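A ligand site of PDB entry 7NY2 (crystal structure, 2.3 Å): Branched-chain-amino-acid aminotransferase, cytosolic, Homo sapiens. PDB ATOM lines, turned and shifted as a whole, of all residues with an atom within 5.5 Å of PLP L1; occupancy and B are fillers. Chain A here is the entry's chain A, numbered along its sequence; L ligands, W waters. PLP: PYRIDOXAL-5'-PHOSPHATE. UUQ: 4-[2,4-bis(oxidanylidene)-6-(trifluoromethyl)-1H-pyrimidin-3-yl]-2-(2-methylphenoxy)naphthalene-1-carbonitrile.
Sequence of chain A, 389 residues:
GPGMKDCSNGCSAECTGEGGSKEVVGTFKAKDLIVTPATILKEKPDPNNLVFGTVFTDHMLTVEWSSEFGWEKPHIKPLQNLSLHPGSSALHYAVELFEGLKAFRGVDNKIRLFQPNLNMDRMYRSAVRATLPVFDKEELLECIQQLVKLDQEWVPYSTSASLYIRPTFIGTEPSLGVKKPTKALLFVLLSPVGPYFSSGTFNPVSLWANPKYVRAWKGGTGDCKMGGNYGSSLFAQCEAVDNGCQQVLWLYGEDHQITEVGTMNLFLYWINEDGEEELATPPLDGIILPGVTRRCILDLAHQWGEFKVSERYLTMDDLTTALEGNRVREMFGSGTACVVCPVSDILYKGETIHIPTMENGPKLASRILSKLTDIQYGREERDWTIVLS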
ATOM      1  N   PHE A  98      11.391  28.873  22.330  1.00  0.00           N
ATOM      2  CA  PHE A  98      11.539  27.448  21.918  1.00  0.00           C
ATOM      3  C   PHE A  98      11.289  27.334  20.407  1.00  0.00           C
ATOM      4  O   PHE A  98      10.930  28.323  19.759  1.00  0.00           O
ATOM      5  CB  PHE A  98      10.576  26.525  22.671  1.00  0.00           C
ATOM      6  CG  PHE A  98       9.098  26.799  22.430  1.00  0.00           C
ATOM      7  CD1 PHE A  98       8.484  27.912  22.977  1.00  0.00           C
ATOM      8  CD2 PHE A  98       8.328  25.934  21.671  1.00  0.00           C
ATOM      9  CE1 PHE A  98       7.149  28.174  22.756  1.00  0.00           C
ATOM     10  CE2 PHE A  98       6.978  26.222  21.442  1.00  0.00           C
ATOM     11  CZ  PHE A  98       6.382  27.323  21.992  1.00  0.00           C
ATOM     12  N   GLY A 100      10.297  23.740  17.490  1.00  0.00           N
ATOM     13  CA  GLY A 100       9.738  22.386  17.308  1.00  0.00           C
ATOM     14  C   GLY A 100       9.888  21.922  15.859  1.00  0.00           C
ATOM     15  O   GLY A 100       9.244  22.532  14.962  1.00  0.00           O
ATOM     16  N   ASN A 119      13.385  26.765  10.653  1.00  0.00           N
ATOM     17  CA  ASN A 119      13.314  26.742  12.134  1.00  0.00           C
ATOM     18  C   ASN A 119      14.460  27.564  12.736  1.00  0.00           C
ATOM     19  O   ASN A 119      14.195  28.330  13.688  1.00  0.00           O
ATOM     20  CB  ASN A 119      13.268  25.323  12.705  1.00  0.00           C
ATOM     21  CG  ASN A 119      11.962  24.638  12.338  1.00  0.00           C
ATOM     22  OD1 ASN A 119      10.910  24.803  13.012  1.00  0.00           O
ATOM     23  ND2 ASN A 119      11.999  23.929  11.219  1.00  0.00           N
ATOM     24  N   ARG A 122      13.717  31.357  12.325  1.00  0.00           N
ATOM     25  CA  ARG A 122      12.637  31.786  13.240  1.00  0.00           C
ATOM     26  C   ARG A 122      13.167  31.852  14.685  1.00  0.00           C
ATOM     27  O   ARG A 122      12.682  32.735  15.445  1.00  0.00           O
ATOM     28  CB  ARG A 122      11.447  30.834  13.124  1.00  0.00           C
ATOM     29  CG  ARG A 122      10.215  31.375  13.846  1.00  0.00           C
ATOM     30  CD  ARG A 122       8.990  30.559  13.510  1.00  0.00           C
ATOM     31  NE  ARG A 122       9.020  29.228  14.086  1.00  0.00           N
ATOM     32  CZ  ARG A 122       8.250  28.214  13.682  1.00  0.00           C
ATOM     33  NH1 ARG A 122       7.422  28.394  12.677  1.00  0.00           N
ATOM     34  NH2 ARG A 122       8.297  27.034  14.268  1.00  0.00           N
ATOM     35  N   ARG A 215      -5.497  35.924  21.647  1.00  0.00           N
ATOM     36  CA  ARG A 215      -4.191  35.211  21.671  1.00  0.00           C
ATOM     37  C   ARG A 215      -3.023  36.203  21.536  1.00  0.00           C
ATOM     38  O   ARG A 215      -1.970  35.954  22.126  1.00  0.00           O
ATOM     39  CB  ARG A 215      -4.125  34.249  20.478  1.00  0.00           C
ATOM     40  CG  ARG A 215      -2.987  33.245  20.596  1.00  0.00           C
ATOM     41  CD  ARG A 215      -2.825  32.466  19.341  1.00  0.00           C
ATOM     42  NE  ARG A 215      -2.124  33.241  18.336  1.00  0.00           N
ATOM     43  CZ  ARG A 215      -0.828  33.417  18.298  1.00  0.00           C
ATOM     44  NH1 ARG A 215      -0.038  32.861  19.204  1.00  0.00           N
ATOM     45  NH2 ARG A 215      -0.326  34.144  17.317  1.00  0.00           N
ATOM     46  N   LYS A 225       8.004  32.681  18.549  1.00  0.00           N
ATOM     47  CA  LYS A 225       7.707  31.501  19.425  1.00  0.00           C
ATOM     48  C   LYS A 225       8.289  31.774  20.816  1.00  0.00           C
ATOM     49  O   LYS A 225       9.203  31.045  21.231  1.00  0.00           O
ATOM     50  CB  LYS A 225       8.161  30.180  18.774  1.00  0.00           C
ATOM     51  CG  LYS A 225       7.036  29.159  18.577  1.00  0.00           C
ATOM     52  CD  LYS A 225       7.420  27.969  17.686  1.00  0.00           C
ATOM     53  CE  LYS A 225       6.416  26.819  17.711  1.00  0.00           C
ATOM     54  NZ  LYS A 225       5.207  27.060  16.885  1.00  0.00           N
ATOM     55  N   TYR A 230       2.027  31.600  25.213  1.00  0.00           N
ATOM     56  CA  TYR A 230       1.394  30.250  25.375  1.00  0.00           C
ATOM     57  C   TYR A 230       0.788  30.098  26.779  1.00  0.00           C
ATOM     58  O   TYR A 230      -0.265  29.448  26.924  1.00  0.00           O
ATOM     59  CB  TYR A 230       2.451  29.168  25.024  1.00  0.00           C
ATOM     60  CG  TYR A 230       2.891  29.336  23.596  1.00  0.00           C
ATOM     61  CD1 TYR A 230       2.129  28.820  22.568  1.00  0.00           C
ATOM     62  CD2 TYR A 230       3.958  30.152  23.263  1.00  0.00           C
ATOM     63  CE1 TYR A 230       2.466  29.060  21.239  1.00  0.00           C
ATOM     64  CE2 TYR A 230       4.302  30.420  21.949  1.00  0.00           C
ATOM     65  CZ  TYR A 230       3.551  29.866  20.933  1.00  0.00           C
ATOM     66  OH  TYR A 230       3.855  30.117  19.626  1.00  0.00           O
ATOM     67  N   GLU A 260      -6.108  31.850  13.965  1.00  0.00           N
ATOM     68  CA  GLU A 260      -5.397  30.578  14.236  1.00  0.00           C
ATOM     69  C   GLU A 260      -6.330  29.577  14.920  1.00  0.00           C
ATOM     70  O   GLU A 260      -7.357  29.998  15.501  1.00  0.00           O
ATOM     71  CB  GLU A 260      -4.114  30.879  15.028  1.00  0.00           C
ATOM     72  CG  GLU A 260      -3.131  31.736  14.224  1.00  0.00           C
ATOM     73  CD  GLU A 260      -1.658  31.479  14.464  1.00  0.00           C
ATOM     74  OE1 GLU A 260      -1.222  30.316  14.385  1.00  0.00           O
ATOM     75  OE2 GLU A 260      -0.929  32.470  14.700  1.00  0.00           O
ATOM     76  N   GLY A 262      -5.946  26.871  17.771  1.00  0.00           N
ATOM     77  CA  GLY A 262      -5.011  26.415  18.839  1.00  0.00           C
ATOM     78  C   GLY A 262      -3.602  26.955  18.571  1.00  0.00           C
ATOM     79  O   GLY A 262      -3.441  28.180  18.428  1.00  0.00           O
ATOM     80  N   THR A 263      -2.617  26.060  18.471  1.00  0.00           N
ATOM     81  CA  THR A 263      -1.238  26.334  17.993  1.00  0.00           C
ATOM     82  C   THR A 263      -1.036  25.789  16.562  1.00  0.00           C
ATOM     83  O   THR A 263       0.088  25.270  16.281  1.00  0.00           O
ATOM     84  CB  THR A 263      -0.236  25.675  18.963  1.00  0.00           C
ATOM     85  OG1 THR A 263      -0.450  24.255  18.994  1.00  0.00           O
ATOM     86  CG2 THR A 263      -0.343  26.225  20.360  1.00  0.00           C
ATOM     87  N   MET A 264      -2.058  25.892  15.691  1.00  0.00           N
ATOM     88  CA  MET A 264      -2.009  25.577  14.225  1.00  0.00           C
ATOM     89  C   MET A 264      -2.464  26.786  13.400  1.00  0.00           C
ATOM     90  O   MET A 264      -3.383  27.482  13.842  1.00  0.00           O
ATOM     91  CB  MET A 264      -2.913  24.386  13.868  1.00  0.00           C
ATOM     92  CG  MET A 264      -2.730  23.219  14.845  1.00  0.00           C
ATOM     93  SD  MET A 264      -3.440  21.609  14.405  1.00  0.00           S
ATOM     94  CE  MET A 264      -5.164  22.020  14.181  1.00  0.00           C
ATOM     95  N   ASN A 265      -1.887  27.002  12.232  1.00  0.00           N
ATOM     96  CA  ASN A 265      -2.291  28.087  11.298  1.00  0.00           C
ATOM     97  C   ASN A 265      -3.613  27.654  10.681  1.00  0.00           C
ATOM     98  O   ASN A 265      -3.842  26.444  10.692  1.00  0.00           O
ATOM     99  CB  ASN A 265      -1.235  28.394  10.228  1.00  0.00           C
ATOM    100  CG  ASN A 265       0.023  29.003  10.801  1.00  0.00           C
ATOM    101  OD1 ASN A 265       1.093  28.400  10.723  1.00  0.00           O
ATOM    102  ND2 ASN A 265      -0.109  30.180  11.397  1.00  0.00           N
ATOM    103  N   LEU A 289       1.604  33.494  13.772  1.00  0.00           N
ATOM    104  CA  LEU A 289       2.915  32.818  13.735  1.00  0.00           C
ATOM    105  C   LEU A 289       3.125  32.296  12.328  1.00  0.00           C
ATOM    106  O   LEU A 289       2.283  31.592  11.794  1.00  0.00           O
ATOM    107  CB  LEU A 289       3.019  31.670  14.757  1.00  0.00           C
ATOM    108  CG  LEU A 289       4.479  31.331  14.999  1.00  0.00           C
ATOM    109  CD1 LEU A 289       4.782  31.262  16.471  1.00  0.00           C
ATOM    110  CD2 LEU A 289       4.900  30.078  14.275  1.00  0.00           C
ATOM    111  N   PRO A 290       4.244  32.666  11.673  1.00  0.00           N
ATOM    112  CA  PRO A 290       4.532  32.150  10.338  1.00  0.00           C
ATOM    113  C   PRO A 290       5.025  30.696  10.448  1.00  0.00           C
ATOM    114  O   PRO A 290       6.232  30.477  10.620  1.00  0.00           O
ATOM    115  CB  PRO A 290       5.537  33.150   9.748  1.00  0.00           C
ATOM    116  CG  PRO A 290       6.043  34.015  10.877  1.00  0.00           C
ATOM    117  CD  PRO A 290       5.218  33.662  12.108  1.00  0.00           C
ATOM    118  N   GLY A 291       4.067  29.757  10.341  1.00  0.00           N
ATOM    119  CA  GLY A 291       4.290  28.302  10.304  1.00  0.00           C
ATOM    120  C   GLY A 291       5.197  27.848   9.159  1.00  0.00           C
ATOM    121  O   GLY A 291       5.181  28.463   8.039  1.00  0.00           O
ATOM    122  N   VAL A 292       5.995  26.812   9.433  1.00  0.00           N
ATOM    123  CA  VAL A 292       6.836  26.117   8.405  1.00  0.00           C
ATOM    124  C   VAL A 292       5.877  25.385   7.458  1.00  0.00           C
ATOM    125  O   VAL A 292       6.080  25.445   6.210  1.00  0.00           O
ATOM    126  CB  VAL A 292       7.856  25.157   9.034  1.00  0.00           C
ATOM    127  CG1 VAL A 292       8.561  24.269   7.977  1.00  0.00           C
ATOM    128  CG2 VAL A 292       8.889  25.922   9.862  1.00  0.00           C
ATOM    129  N   THR A 293       4.868  24.710   8.009  1.00  0.00           N
ATOM    130  CA  THR A 293       3.838  24.014   7.196  1.00  0.00           C
ATOM    131  C   THR A 293       3.060  25.066   6.388  1.00  0.00           C
ATOM    132  O   THR A 293       2.808  24.810   5.190  1.00  0.00           O
ATOM    133  CB  THR A 293       2.926  23.161   8.084  1.00  0.00           C
ATOM    134  OG1 THR A 293       3.663  22.572   9.163  1.00  0.00           O
ATOM    135  CG2 THR A 293       2.300  22.024   7.328  1.00  0.00           C
ATOM    136  N   ARG A 294       2.715  26.213   6.985  1.00  0.00           N
ATOM    137  CA  ARG A 294       1.957  27.289   6.291  1.00  0.00           C
ATOM    138  C   ARG A 294       2.794  27.755   5.074  1.00  0.00           C
ATOM    139  O   ARG A 294       2.200  27.869   3.967  1.00  0.00           O
ATOM    140  CB  ARG A 294       1.571  28.403   7.267  1.00  0.00           C
ATOM    141  CG  ARG A 294       1.061  29.693   6.622  1.00  0.00           C
ATOM    142  CD  ARG A 294       0.982  30.837   7.629  1.00  0.00           C
ATOM    143  NE  ARG A 294       0.368  32.021   7.054  1.00  0.00           N
ATOM    144  CZ  ARG A 294       0.962  32.879   6.213  1.00  0.00           C
ATOM    145  NH1 ARG A 294       2.223  32.733   5.842  1.00  0.00           N
ATOM    146  NH2 ARG A 294       0.262  33.892   5.741  1.00  0.00           N
ATOM    147  N   SER A 334      -2.988  23.737  10.166  1.00  0.00           N
ATOM    148  CA  SER A 334      -1.657  23.250   9.690  1.00  0.00           C
ATOM    149  C   SER A 334      -0.592  23.395  10.794  1.00  0.00           C
ATOM    150  O   SER A 334      -0.493  24.433  11.339  1.00  0.00           O
ATOM    151  CB  SER A 334      -1.240  23.959   8.367  1.00  0.00           C
ATOM    152  OG  SER A 334      -0.801  25.295   8.591  1.00  0.00           O
ATOM    153  N   GLY A 335       0.257  22.416  11.012  1.00  0.00           N
ATOM    154  CA  GLY A 335       1.527  22.635  11.748  1.00  0.00           C
ATOM    155  C   GLY A 335       2.437  21.429  11.764  1.00  0.00           C
ATOM    156  O   GLY A 335       2.143  20.464  11.056  1.00  0.00           O
ATOM    157  N   THR A 336       3.516  21.462  12.563  1.00  0.00           N
ATOM    158  CA  THR A 336       4.424  20.306  12.721  1.00  0.00           C
ATOM    159  C   THR A 336       3.646  19.151  13.356  1.00  0.00           C
ATOM    160  O   THR A 336       3.913  17.978  13.007  1.00  0.00           O
ATOM    161  CB  THR A 336       5.694  20.679  13.485  1.00  0.00           C
ATOM    162  OG1 THR A 336       6.408  21.482  12.539  1.00  0.00           O
ATOM    163  CG2 THR A 336       6.545  19.500  13.913  1.00  0.00           C
ATOM    164  N   ALA A 337       2.674  19.495  14.197  1.00  0.00           N
ATOM    165  CA  ALA A 337       1.908  18.518  15.008  1.00  0.00           C
ATOM    166  C   ALA A 337       1.176  17.529  14.107  1.00  0.00           C
ATOM    167  O   ALA A 337       1.445  16.323  14.189  1.00  0.00           O
ATOM    168  CB  ALA A 337       0.942  19.277  15.881  1.00  0.00           C
HETATM  169  N1  PLP L   1       0.684  28.577  15.325  1.00  0.00           N
HETATM  170  C2  PLP L   1       1.360  28.821  16.457  1.00  0.00           C
HETATM  171  C2A PLP L   1       0.811  29.837  17.402  1.00  0.00           C
HETATM  172  C3  PLP L   1       2.548  28.143  16.735  1.00  0.00           C
HETATM  173  O3  PLP L   1       3.195  28.410  17.884  1.00  0.00           O
HETATM  174  C4  PLP L   1       3.044  27.181  15.828  1.00  0.00           C
HETATM  175  C4A PLP L   1       4.299  26.498  16.163  1.00  0.00           C
HETATM  176  C5  PLP L   1       2.307  26.946  14.652  1.00  0.00           C
HETATM  177  C6  PLP L   1       1.153  27.654  14.454  1.00  0.00           C
HETATM  178  C5A PLP L   1       2.731  25.934  13.623  1.00  0.00           C
HETATM  179  O4P PLP L   1       4.060  26.232  13.107  1.00  0.00           O
HETATM  180  P   PLP L   1       4.890  25.042  12.338  1.00  0.00           P
HETATM  181  O1P PLP L   1       4.870  23.817  13.254  1.00  0.00           O
HETATM  182  O2P PLP L   1       6.228  25.672  12.199  1.00  0.00           O
HETATM  183  O3P PLP L   1       4.187  24.775  11.048  1.00  0.00           O
HETATM  184  C4  UUQ L   2       0.539  18.244  20.026  1.00  0.00           C
HETATM  185  C5  UUQ L   2       1.683  17.914  19.306  1.00  0.00           C
HETATM  186  C6  UUQ L   2       2.586  18.920  18.928  1.00  0.00           C
HETATM  187  C7  UUQ L   2      -0.379  17.239  20.394  1.00  0.00           C
HETATM  188  C8  UUQ L   2      -0.164  15.912  20.037  1.00  0.00           C
HETATM  189  C10 UUQ L   2       1.890  16.589  18.928  1.00  0.00           C
HETATM  190  N12 UUQ L   2      -0.840  19.949  21.085  1.00  0.00           N
HETATM  191  C15 UUQ L   2       3.427  22.471  19.405  1.00  0.00           C
HETATM  192  C17 UUQ L   2       3.771  23.989  21.283  1.00  0.00           C
HETATM  193  C20 UUQ L   2       3.235  23.583  18.560  1.00  0.00           C
HETATM  194  C21 UUQ L   2       3.910  21.534  21.765  1.00  0.00           C
HETATM  195  C22 UUQ L   2      -2.025  20.075  20.365  1.00  0.00           C
HETATM  196  C28 UUQ L   2      -3.210  20.706  22.348  1.00  0.00           C
HETATM  197  C16 UUQ L   2       3.699  22.697  20.779  1.00  0.00           C
HETATM  198  C18 UUQ L   2       3.560  25.089  20.434  1.00  0.00           C
HETATM  199  C19 UUQ L   2       3.298  24.878  19.067  1.00  0.00           C
HETATM  200  O13 UUQ L   2       3.348  21.208  18.849  1.00  0.00           O
HETATM  201  C1  UUQ L   2       2.381  20.266  19.259  1.00  0.00           C
HETATM  202  C2  UUQ L   2       1.231  20.591  20.000  1.00  0.00           C
HETATM  203  C11 UUQ L   2       3.734  18.552  18.175  1.00  0.00           C
HETATM  204  N14 UUQ L   2       4.664  18.293  17.570  1.00  0.00           N
HETATM  205  C9  UUQ L   2       0.982  15.599  19.304  1.00  0.00           C
HETATM  206  C3  UUQ L   2       0.319  19.588  20.381  1.00  0.00           C
HETATM  207  C25 UUQ L   2      -0.853  20.196  22.453  1.00  0.00           C
HETATM  208  O26 UUQ L   2       0.173  20.090  23.102  1.00  0.00           O
HETATM  209  C27 UUQ L   2      -2.039  20.578  23.092  1.00  0.00           C
HETATM  210  C29 UUQ L   2      -4.564  21.110  22.954  1.00  0.00           C
HETATM  211  F31 UUQ L   2      -4.510  21.357  24.255  1.00  0.00           F
HETATM  212  F32 UUQ L   2      -5.023  22.193  22.325  1.00  0.00           F
HETATM  213  F30 UUQ L   2      -5.377  20.081  22.755  1.00  0.00           F
HETATM  214  N23 UUQ L   2      -3.177  20.441  20.991  1.00  0.00           N
HETATM  215  O24 UUQ L   2      -2.060  19.856  19.169  1.00  0.00           O
HETATM  216  O   HOH W   1       6.413  23.889  15.124  1.00  0.00           O
HETATM  217  O   HOH W   2       8.400  23.809  12.149  1.00  0.00           O
HETATM  218  O   HOH W   3       1.832  26.023   9.751  1.00  0.00           O
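The side-chain hydroxyl (OG1) of Thr 336 sits at hydrogen-bond distance from an oxygen (O1P) of PLP L1 (2.9 Å). O3P of PLP L1 sits at hydrogen-bond distance from OG1 of Thr 293 (2.9 Å). The guanidinium group (NH1) of Arg 122 lies within salt-bridge range of an oxygen (O2P) of PLP L1, at 3.0 Å. OH of Tyr 230 lies within hydrogen-bond range of O3 of PLP L1, 2.5 Å away. OE1 of Glu 260 lies within hydrogen-bond range of N1 of PLP L1 (2.7 Å). The backbone NH of Thr 336 lies within hydrogen-bond range of an oxygen (O1P) of PLP L1. A carbon (C4A) of PLP L1 is bonded to the side-chain amino group (NZ) of Lys 225 (1.3 Å). An oxygen (O3P) of PLP L1 is in hydrogen-bond range of the backbone NH of Thr 293 (3.1 Å). O2P of PLP L1 is in hydrogen-bond range of N of Val 292 (3.0 Å).
The side-chain amide nitrogen (ND2) of Asn 265 sits at hydrogen-bond distance from the backbone carbonyl oxygen (O) of Leu 289 (2.8 Å). OG1 of Thr 293 sits close to O of Gly 335 (3.2 Å). The backbone NH (N) of Leu 289 is in hydrogen-bond range of the side-chain carboxylate (OE2) of Glu 260 (2.9 Å). O of Asn 265 is in hydrogen-bond range of N of Ser 334, 2.9 Å away. The backbone NH of Phe 98 lies within hydrogen-bond range of the backbone carbonyl oxygen of Lys 225 (3.3 Å). The side-chain carboxylate (OE2) of Glu 260 lies within salt-bridge range of the guanidinium group (NH2) of Arg 215. The side-chain amide nitrogen (ND2) of Asn 265 lies within hydrogen-bond range of the side-chain carboxylate (OE1) of Glu 260 (3.2 Å). N of Gly 291 lies close to OD1 of Asn 265 (3.3 Å).
N1 of PLP L1 lies close to O of Thr 263 (3.5 Å). NH1 of Arg 215 touches C2A of PLP L1, 3.6 Å away. Met 264 touches PLP L1 (CA to C6, 3.8 Å). OD1 of Asn 265 touches C6 of PLP L1, at 3.8 Å. Leu 289 touches PLP L1 (CD1 to O3, 3.6 Å). CA of Gly 291 touches O4P of PLP L1 (3.5 Å). CA of Gly 335 touches O3P of PLP L1, at 3.5 Å. Within 4 Å of PLP L1: Arg 122, Arg 215, Lys 225, Tyr 230, Glu 260, Thr 263, Met 264, Asn 265, Leu 289, Gly 291, Val 292, Thr 293, Gly 335 and Thr 336. The nearest printed residue that does not touch PLP L1 is Ser 334 (4.2 Å).
Water W1 bridges O1P of PLP L1 (2.4 Å) and O of Gly 100 (3.1 Å). Water W2 lies within hydrogen-bond range of the side-chain amide oxygen (OD1) of Asn 119, an oxygen (O2P) of PLP L1, the side-chain hydroxyl (OG1) of Thr 336 and the backbone carbonyl oxygen (O) of Gly 100. Water W3 lies within hydrogen-bond range of the side-chain amide oxygen of Asn 265 (2.7 Å), the backbone NH of Arg 294 (2.9 Å), an oxygen (O3P) of PLP L1 (3.0 Å) and the side-chain hydroxyl of Ser 334 (3.0 Å).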
